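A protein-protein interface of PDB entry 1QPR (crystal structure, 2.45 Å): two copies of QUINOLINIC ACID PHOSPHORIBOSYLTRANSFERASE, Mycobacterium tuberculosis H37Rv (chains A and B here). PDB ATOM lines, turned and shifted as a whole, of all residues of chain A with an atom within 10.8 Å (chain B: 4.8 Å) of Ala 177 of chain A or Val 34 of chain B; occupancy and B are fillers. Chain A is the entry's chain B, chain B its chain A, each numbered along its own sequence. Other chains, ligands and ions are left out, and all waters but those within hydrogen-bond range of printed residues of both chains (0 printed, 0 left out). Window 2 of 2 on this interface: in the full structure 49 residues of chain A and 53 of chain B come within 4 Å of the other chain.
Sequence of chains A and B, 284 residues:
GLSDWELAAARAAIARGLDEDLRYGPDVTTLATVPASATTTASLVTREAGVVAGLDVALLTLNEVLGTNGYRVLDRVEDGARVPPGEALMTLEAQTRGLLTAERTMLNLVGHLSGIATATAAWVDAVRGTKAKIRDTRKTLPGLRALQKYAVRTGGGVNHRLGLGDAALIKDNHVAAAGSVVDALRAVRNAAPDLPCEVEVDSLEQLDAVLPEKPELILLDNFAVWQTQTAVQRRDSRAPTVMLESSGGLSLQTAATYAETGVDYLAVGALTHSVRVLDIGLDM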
ATOM      1  N   LEU A 169      -4.443   6.364 -12.152  1.00  0.00           N
ATOM      2  CA  LEU A 169      -5.619   5.560 -11.889  1.00  0.00           C
ATOM      3  C   LEU A 169      -5.333   4.815 -10.606  1.00  0.00           C
ATOM      4  O   LEU A 169      -4.692   3.772 -10.613  1.00  0.00           O
ATOM      5  CB  LEU A 169      -5.877   4.573 -13.018  1.00  0.00           C
ATOM      6  CG  LEU A 169      -7.355   4.241 -13.248  1.00  0.00           C
ATOM      7  CD1 LEU A 169      -7.509   3.289 -14.423  1.00  0.00           C
ATOM      8  CD2 LEU A 169      -7.991   3.671 -12.007  1.00  0.00           C
ATOM      9  N   ILE A 170      -5.818   5.351  -9.505  1.00  0.00           N
ATOM     10  CA  ILE A 170      -5.593   4.741  -8.217  1.00  0.00           C
ATOM     11  C   ILE A 170      -6.456   3.501  -8.063  1.00  0.00           C
ATOM     12  O   ILE A 170      -7.680   3.596  -8.043  1.00  0.00           O
ATOM     13  CB  ILE A 170      -5.880   5.754  -7.083  1.00  0.00           C
ATOM     14  CG1 ILE A 170      -5.062   7.032  -7.323  1.00  0.00           C
ATOM     15  CG2 ILE A 170      -5.504   5.161  -5.762  1.00  0.00           C
ATOM     16  CD1 ILE A 170      -5.417   8.195  -6.470  1.00  0.00           C
ATOM     17  N   LYS A 171      -5.807   2.338  -7.990  1.00  0.00           N
ATOM     18  CA  LYS A 171      -6.479   1.038  -7.847  1.00  0.00           C
ATOM     19  C   LYS A 171      -6.512   0.488  -6.437  1.00  0.00           C
ATOM     20  O   LYS A 171      -5.826   0.988  -5.564  1.00  0.00           O
ATOM     21  CB  LYS A 171      -5.809   0.023  -8.759  1.00  0.00           C
ATOM     22  CG  LYS A 171      -6.071   0.320 -10.226  1.00  0.00           C
ATOM     23  CD  LYS A 171      -5.198  -0.493 -11.163  1.00  0.00           C
ATOM     24  CE  LYS A 171      -5.661  -0.339 -12.611  1.00  0.00           C
ATOM     25  NZ  LYS A 171      -7.008  -0.967 -12.788  1.00  0.00           N
ATOM     26  N   ASP A 172      -7.247  -0.598  -6.241  1.00  0.00           N
ATOM     27  CA  ASP A 172      -7.355  -1.227  -4.931  1.00  0.00           C
ATOM     28  C   ASP A 172      -6.023  -1.557  -4.250  1.00  0.00           C
ATOM     29  O   ASP A 172      -5.887  -1.431  -3.011  1.00  0.00           O
ATOM     30  CB  ASP A 172      -8.242  -2.484  -5.001  1.00  0.00           C
ATOM     31  CG  ASP A 172      -7.898  -3.406  -6.160  1.00  0.00           C
ATOM     32  OD1 ASP A 172      -7.028  -3.068  -6.988  1.00  0.00           O
ATOM     33  OD2 ASP A 172      -8.533  -4.481  -6.252  1.00  0.00           O
ATOM     34  N   ASN A 173      -5.044  -1.959  -5.063  1.00  0.00           N
ATOM     35  CA  ASN A 173      -3.720  -2.311  -4.556  1.00  0.00           C
ATOM     36  C   ASN A 173      -2.922  -1.096  -4.102  1.00  0.00           C
ATOM     37  O   ASN A 173      -2.075  -1.208  -3.210  1.00  0.00           O
ATOM     38  CB  ASN A 173      -2.966  -3.153  -5.575  1.00  0.00           C
ATOM     39  CG  ASN A 173      -3.455  -4.604  -5.602  1.00  0.00           C
ATOM     40  OD1 ASN A 173      -3.873  -5.136  -4.585  1.00  0.00           O
ATOM     41  ND2 ASN A 173      -3.397  -5.248  -6.765  1.00  0.00           N
ATOM     42  N   HIS A 174      -3.250   0.074  -4.650  1.00  0.00           N
ATOM     43  CA  HIS A 174      -2.578   1.321  -4.267  1.00  0.00           C
ATOM     44  C   HIS A 174      -3.124   1.802  -2.958  1.00  0.00           C
ATOM     45  O   HIS A 174      -2.390   2.273  -2.107  1.00  0.00           O
ATOM     46  CB  HIS A 174      -2.837   2.416  -5.282  1.00  0.00           C
ATOM     47  CG  HIS A 174      -2.242   2.134  -6.611  1.00  0.00           C
ATOM     48  ND1 HIS A 174      -0.895   1.911  -6.782  1.00  0.00           N
ATOM     49  CD2 HIS A 174      -2.811   2.001  -7.831  1.00  0.00           C
ATOM     50  CE1 HIS A 174      -0.659   1.648  -8.056  1.00  0.00           C
ATOM     51  NE2 HIS A 174      -1.806   1.696  -8.713  1.00  0.00           N
ATOM     52  N   VAL A 175      -4.453   1.810  -2.886  1.00  0.00           N
ATOM     53  CA  VAL A 175      -5.216   2.215  -1.698  1.00  0.00           C
ATOM     54  C   VAL A 175      -4.727   1.376  -0.514  1.00  0.00           C
ATOM     55  O   VAL A 175      -4.498   1.923   0.568  1.00  0.00           O
ATOM     56  CB  VAL A 175      -6.761   1.993  -1.910  1.00  0.00           C
ATOM     57  CG1 VAL A 175      -7.502   2.146  -0.604  1.00  0.00           C
ATOM     58  CG2 VAL A 175      -7.310   2.987  -2.943  1.00  0.00           C
ATOM     59  N   ALA A 176      -4.558   0.065  -0.742  1.00  0.00           N
ATOM     60  CA  ALA A 176      -4.050  -0.892   0.259  1.00  0.00           C
ATOM     61  C   ALA A 176      -2.665  -0.425   0.753  1.00  0.00           C
ATOM     62  O   ALA A 176      -2.426  -0.294   1.967  1.00  0.00           O
ATOM     63  CB  ALA A 176      -3.927  -2.294  -0.365  1.00  0.00           C
ATOM     64  N   ALA A 177      -1.772  -0.150  -0.204  1.00  0.00           N
ATOM     65  CA  ALA A 177      -0.423   0.313   0.081  1.00  0.00           C
ATOM     66  C   ALA A 177      -0.405   1.719   0.713  1.00  0.00           C
ATOM     67  O   ALA A 177       0.364   1.968   1.627  1.00  0.00           O
ATOM     68  CB  ALA A 177       0.408   0.272  -1.205  1.00  0.00           C
ATOM     69  N   ALA A 178      -1.267   2.626   0.255  1.00  0.00           N
ATOM     70  CA  ALA A 178      -1.323   3.991   0.789  1.00  0.00           C
ATOM     71  C   ALA A 178      -2.162   4.071   2.061  1.00  0.00           C
ATOM     72  O   ALA A 178      -2.244   5.130   2.704  1.00  0.00           O
ATOM     73  CB  ALA A 178      -1.894   4.933  -0.247  1.00  0.00           C
ATOM     74  N   GLY A 179      -2.849   2.977   2.374  1.00  0.00           N
ATOM     75  CA  GLY A 179      -3.680   2.938   3.565  1.00  0.00           C
ATOM     76  C   GLY A 179      -5.058   3.594   3.492  1.00  0.00           C
ATOM     77  O   GLY A 179      -5.901   3.338   4.365  1.00  0.00           O
ATOM     78  N   SER A 180      -5.306   4.439   2.493  1.00  0.00           N
ATOM     79  CA  SER A 180      -6.609   5.086   2.380  1.00  0.00           C
ATOM     80  C   SER A 180      -6.767   5.701   1.008  1.00  0.00           C
ATOM     81  O   SER A 180      -5.778   6.179   0.444  1.00  0.00           O
ATOM     82  CB  SER A 180      -6.740   6.159   3.464  1.00  0.00           C
ATOM     83  OG  SER A 180      -7.580   7.237   3.074  1.00  0.00           O
ATOM     84  N   VAL A 181      -7.991   5.688   0.469  1.00  0.00           N
ATOM     85  CA  VAL A 181      -8.239   6.279  -0.847  1.00  0.00           C
ATOM     86  C   VAL A 181      -7.945   7.757  -0.875  1.00  0.00           C
ATOM     87  O   VAL A 181      -7.386   8.249  -1.844  1.00  0.00           O
ATOM     88  CB  VAL A 181      -9.677   6.117  -1.364  1.00  0.00           C
ATOM     89  CG1 VAL A 181      -9.855   4.767  -1.966  1.00  0.00           C
ATOM     90  CG2 VAL A 181     -10.667   6.353  -0.272  1.00  0.00           C
ATOM     91  N   VAL A 182      -8.327   8.478   0.169  1.00  0.00           N
ATOM     92  CA  VAL A 182      -8.074   9.912   0.189  1.00  0.00           C
ATOM     93  C   VAL A 182      -6.574  10.224   0.320  1.00  0.00           C
ATOM     94  O   VAL A 182      -6.085  11.217  -0.248  1.00  0.00           O
ATOM     95  CB  VAL A 182      -8.862  10.592   1.305  1.00  0.00           C
ATOM     96  CG1 VAL A 182      -8.628  12.112   1.279  1.00  0.00           C
ATOM     97  CG2 VAL A 182     -10.322  10.256   1.145  1.00  0.00           C
ATOM     98  N   ASP A 183      -5.852   9.351   1.034  1.00  0.00           N
ATOM     99  CA  ASP A 183      -4.416   9.506   1.241  1.00  0.00           C
ATOM    100  C   ASP A 183      -3.722   9.335  -0.088  1.00  0.00           C
ATOM    101  O   ASP A 183      -2.969  10.202  -0.515  1.00  0.00           O
ATOM    102  CB  ASP A 183      -3.895   8.476   2.249  1.00  0.00           C
ATOM    103  CG  ASP A 183      -4.216   8.847   3.703  1.00  0.00           C
ATOM    104  OD1 ASP A 183      -4.625  10.006   3.979  1.00  0.00           O
ATOM    105  OD2 ASP A 183      -4.029   7.968   4.577  1.00  0.00           O
ATOM    106  N   ALA A 184      -4.030   8.227  -0.756  1.00  0.00           N
ATOM    107  CA  ALA A 184      -3.502   7.905  -2.074  1.00  0.00           C
ATOM    108  C   ALA A 184      -3.806   9.026  -3.101  1.00  0.00           C
ATOM    109  O   ALA A 184      -2.927   9.450  -3.855  1.00  0.00           O
ATOM    110  CB  ALA A 184      -4.097   6.583  -2.529  1.00  0.00           C
ATOM    111  N   LEU A 185      -5.038   9.519  -3.107  1.00  0.00           N
ATOM    112  CA  LEU A 185      -5.439  10.586  -4.024  1.00  0.00           C
ATOM    113  C   LEU A 185      -4.560  11.779  -3.780  1.00  0.00           C
ATOM    114  O   LEU A 185      -3.993  12.345  -4.705  1.00  0.00           O
ATOM    115  CB  LEU A 185      -6.897  11.009  -3.785  1.00  0.00           C
ATOM    116  CG  LEU A 185      -7.721  11.446  -4.999  1.00  0.00           C
ATOM    117  CD1 LEU A 185      -9.070  11.977  -4.552  1.00  0.00           C
ATOM    118  CD2 LEU A 185      -6.990  12.478  -5.810  1.00  0.00           C
ATOM    119  N   ALA A 187      -1.655  11.944  -2.414  1.00  0.00           N
ATOM    120  CA  ALA A 187      -0.281  11.649  -2.833  1.00  0.00           C
ATOM    121  C   ALA A 187      -0.092  11.817  -4.325  1.00  0.00           C
ATOM    122  O   ALA A 187       0.854  12.476  -4.754  1.00  0.00           O
ATOM    123  CB  ALA A 187       0.134  10.243  -2.417  1.00  0.00           C
ATOM    124  N   VAL A 188      -1.002  11.247  -5.114  1.00  0.00           N
ATOM    125  CA  VAL A 188      -0.916  11.348  -6.561  1.00  0.00           C
ATOM    126  C   VAL A 188      -1.050  12.789  -7.009  1.00  0.00           C
ATOM    127  O   VAL A 188      -0.340  13.223  -7.914  1.00  0.00           O
ATOM    128  CB  VAL A 188      -1.968  10.479  -7.255  1.00  0.00           C
ATOM    129  CG1 VAL A 188      -2.071  10.852  -8.723  1.00  0.00           C
ATOM    130  CG2 VAL A 188      -1.574   8.996  -7.129  1.00  0.00           C
ATOM    131  N   ALA A 191       2.284  14.629  -6.335  1.00  0.00           N
ATOM    132  CA  ALA A 191       3.346  14.153  -7.215  1.00  0.00           C
ATOM    133  C   ALA A 191       3.152  14.491  -8.688  1.00  0.00           C
ATOM    134  O   ALA A 191       4.106  14.827  -9.363  1.00  0.00           O
ATOM    135  CB  ALA A 191       3.538  12.654  -7.036  1.00  0.00           C
ATOM    136  N   THR B  30       2.068   4.354  -8.731  1.00  0.00           N
ATOM    137  CA  THR B  30       2.752   3.404  -7.815  1.00  0.00           C
ATOM    138  C   THR B  30       3.898   4.072  -7.080  1.00  0.00           C
ATOM    139  O   THR B  30       4.090   3.852  -5.891  1.00  0.00           O
ATOM    140  CB  THR B  30       3.345   2.174  -8.551  1.00  0.00           C
ATOM    141  OG1 THR B  30       2.286   1.441  -9.166  1.00  0.00           O
ATOM    142  CG2 THR B  30       4.104   1.251  -7.592  1.00  0.00           C
ATOM    143  N   LEU B  31       4.673   4.863  -7.817  1.00  0.00           N
ATOM    144  CA  LEU B  31       5.817   5.580  -7.268  1.00  0.00           C
ATOM    145  C   LEU B  31       5.347   6.524  -6.191  1.00  0.00           C
ATOM    146  O   LEU B  31       6.013   6.699  -5.174  1.00  0.00           O
ATOM    147  CB  LEU B  31       6.511   6.387  -8.360  1.00  0.00           C
ATOM    148  CG  LEU B  31       7.671   5.753  -9.128  1.00  0.00           C
ATOM    149  CD1 LEU B  31       7.608   4.268  -9.158  1.00  0.00           C
ATOM    150  CD2 LEU B  31       7.650   6.301 -10.523  1.00  0.00           C
ATOM    151  N   ALA B  32       4.215   7.163  -6.443  1.00  0.00           N
ATOM    152  CA  ALA B  32       3.654   8.083  -5.469  1.00  0.00           C
ATOM    153  C   ALA B  32       3.005   7.420  -4.233  1.00  0.00           C
ATOM    154  O   ALA B  32       3.120   7.936  -3.124  1.00  0.00           O
ATOM    155  CB  ALA B  32       2.658   8.992  -6.145  1.00  0.00           C
ATOM    156  N   THR B  33       2.327   6.289  -4.416  1.00  0.00           N
ATOM    157  CA  THR B  33       1.645   5.613  -3.299  1.00  0.00           C
ATOM    158  C   THR B  33       2.431   4.546  -2.504  1.00  0.00           C
ATOM    159  O   THR B  33       2.170   4.349  -1.308  1.00  0.00           O
ATOM    160  CB  THR B  33       0.282   5.006  -3.758  1.00  0.00           C
ATOM    161  OG1 THR B  33       0.503   3.919  -4.681  1.00  0.00           O
ATOM    162  CG2 THR B  33      -0.550   6.058  -4.454  1.00  0.00           C
ATOM    163  N   VAL B  34       3.367   3.845  -3.144  1.00  0.00           N
ATOM    164  CA  VAL B  34       4.123   2.828  -2.433  1.00  0.00           C
ATOM    165  C   VAL B  34       5.616   3.066  -2.392  1.00  0.00           C
ATOM    166  O   VAL B  34       6.207   3.514  -3.355  1.00  0.00           O
ATOM    167  CB  VAL B  34       3.763   1.388  -2.901  1.00  0.00           C
ATOM    168  CG1 VAL B  34       3.225   1.407  -4.285  1.00  0.00           C
ATOM    169  CG2 VAL B  34       4.938   0.446  -2.791  1.00  0.00           C
ATOM    170  N   PRO B  35       6.205   2.935  -1.195  1.00  0.00           N
ATOM    171  CA  PRO B  35       7.633   3.122  -0.978  1.00  0.00           C
ATOM    172  C   PRO B  35       8.512   2.039  -1.609  1.00  0.00           C
ATOM    173  O   PRO B  35       8.114   0.890  -1.765  1.00  0.00           O
ATOM    174  CB  PRO B  35       7.738   3.133   0.553  1.00  0.00           C
ATOM    175  CG  PRO B  35       6.583   2.349   1.016  1.00  0.00           C
ATOM    176  CD  PRO B  35       5.504   2.859   0.104  1.00  0.00           C
ATOM    177  N   ALA B  36       9.754   2.392  -1.881  1.00  0.00           N
ATOM    178  CA  ALA B  36      10.667   1.461  -2.504  1.00  0.00           C
ATOM    179  C   ALA B  36      10.950   0.239  -1.650  1.00  0.00           C
ATOM    180  O   ALA B  36      11.231  -0.845  -2.162  1.00  0.00           O
ATOM    181  CB  ALA B  36      11.955   2.163  -2.863  1.00  0.00           C
ATOM    182  N   ALA B  38       8.816  -1.248   0.214  1.00  0.00           N
ATOM    183  CA  ALA B  38       7.612  -2.044   0.400  1.00  0.00           C
ATOM    184  C   ALA B  38       7.756  -3.448  -0.169  1.00  0.00           C
ATOM    185  O   ALA B  38       8.368  -3.654  -1.217  1.00  0.00           O
ATOM    186  CB  ALA B  38       6.434  -1.359  -0.208  1.00  0.00           C
ATOM    187  N   THR B  96       6.743  -4.518  -3.624  1.00  0.00           N
ATOM    188  CA  THR B  96       5.443  -4.076  -4.040  1.00  0.00           C
ATOM    189  C   THR B  96       5.481  -3.259  -5.305  1.00  0.00           C
ATOM    190  O   THR B  96       4.740  -3.539  -6.231  1.00  0.00           O
ATOM    191  CB  THR B  96       4.759  -3.308  -2.896  1.00  0.00           C
ATOM    192  OG1 THR B  96       4.811  -4.113  -1.709  1.00  0.00           O
ATOM    193  CG2 THR B  96       3.325  -3.026  -3.211  1.00  0.00           C
ATOM    194  N   ARG B  97       6.386  -2.296  -5.400  1.00  0.00           N
ATOM    195  CA  ARG B  97       6.426  -1.462  -6.606  1.00  0.00           C
ATOM    196  C   ARG B  97       6.558  -2.284  -7.889  1.00  0.00           C
ATOM    197  O   ARG B  97       5.898  -2.013  -8.886  1.00  0.00           O
ATOM    198  CB  ARG B  97       7.573  -0.459  -6.536  1.00  0.00           C
ATOM    199  CG  ARG B  97       7.299   0.741  -5.675  1.00  0.00           C
ATOM    200  CD  ARG B  97       8.492   1.681  -5.663  1.00  0.00           C
ATOM    201  NE  ARG B  97       8.166   2.978  -5.070  1.00  0.00           N
ATOM    202  CZ  ARG B  97       8.973   4.037  -5.047  1.00  0.00           C
ATOM    203  NH1 ARG B  97      10.183   3.981  -5.566  1.00  0.00           N
ATOM    204  NH2 ARG B  97       8.535   5.184  -4.580  1.00  0.00           N
ATOM    205  N   LEU B 100       3.136  -4.208  -8.838  1.00  0.00           N
ATOM    206  CA  LEU B 100       2.089  -3.351  -9.369  1.00  0.00           C
ATOM    207  C   LEU B 100       2.327  -2.885 -10.795  1.00  0.00           C
ATOM    208  O   LEU B 100       1.405  -2.610 -11.563  1.00  0.00           O
ATOM    209  CB  LEU B 100       1.883  -2.179  -8.410  1.00  0.00           C
ATOM    210  CG  LEU B 100       0.827  -2.355  -7.307  1.00  0.00           C
ATOM    211  CD1 LEU B 100       0.684  -3.784  -6.918  1.00  0.00           C
ATOM    212  CD2 LEU B 100       1.138  -1.497  -6.123  1.00  0.00           C
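No position is printed for both chains.
Of the 6 pairs that touch across the chains among the printed residues, none has its exchanged pair printed and touching as well.
Of the 11 printed residues of chain B, 5 touch a printed residue of chain A.
Hydrophobic or aromatic side chains of chain B within 4 Å of the printed part of chain A: Ala 32, Val 34 and Leu 100.
Of the 20 printed residues of chain A, 5 touch a printed residue of chain B.
Hydrophobic or aromatic side chains of chain A that line the printed part of chain B: His 174, Ala 177, Ala 187 and Ala 191.
Along chain A the printed residues that touch a printed residue of chain B span positions 173 to 191.
Among the printed residues, 6 pairs touch across the chains.
The guanidinium group (NE) of Arg 97 of chain B sits at hydrogen-bond distance from the backbone carbonyl oxygen (O) of Val 34 of chain B (2.7 Å).
ND1 of His 174 of chain A is in hydrogen-bond range of OG1 of Thr 33 of chain B, at 3.2 Å.
Printed residues of chain B within 4 Å of Asn 173 of chain A: Leu 100.
Of the printed residues of chain B, His 174 of chain A touches Thr 30 and Thr 33.
Ala 177 of chain A touches just one residue of chain B: Val 34 (3.9 Å).
Printed residues of chain B within 4 Å of Ala 187 of chain A: Ala 32.
Leu 31 of chain B touches none of the printed residues of chain A.
Of chain A, only Ala 187 and Ala 191 come within 4 Å of Ala 32 of chain B.
Thr 33 of chain B touches one residue of chain A.
Val 34 of chain B touches just one residue of chain A: Ala 177 (3.9 Å).
No residue of chain A comes within 4 Å of Ala 36 of chain B.
No residue of chain A comes within 4 Å of Ala 38 of chain B.
No residue of chain A comes within 4 Å of Thr 96 of chain B.
The nearest residue of chain B that does not touch Ala 177 of chain A is Thr 33 of chain B (4.2 Å).
The nearest residue of chain A that does not touch Val 34 of chain B is His 174 of chain A (4.8 Å).
Among the printed residues, pairs that only touch across the chains: His 174 of chain A with Thr 30 of chain B, Ala 187 of chain A with Ala 32 of chain B, Ala 191 of chain A with Ala 32 of chain B, Ala 177 of chain A with Val 34 of chain B and Asn 173 of chain A with Leu 100 of chain B.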
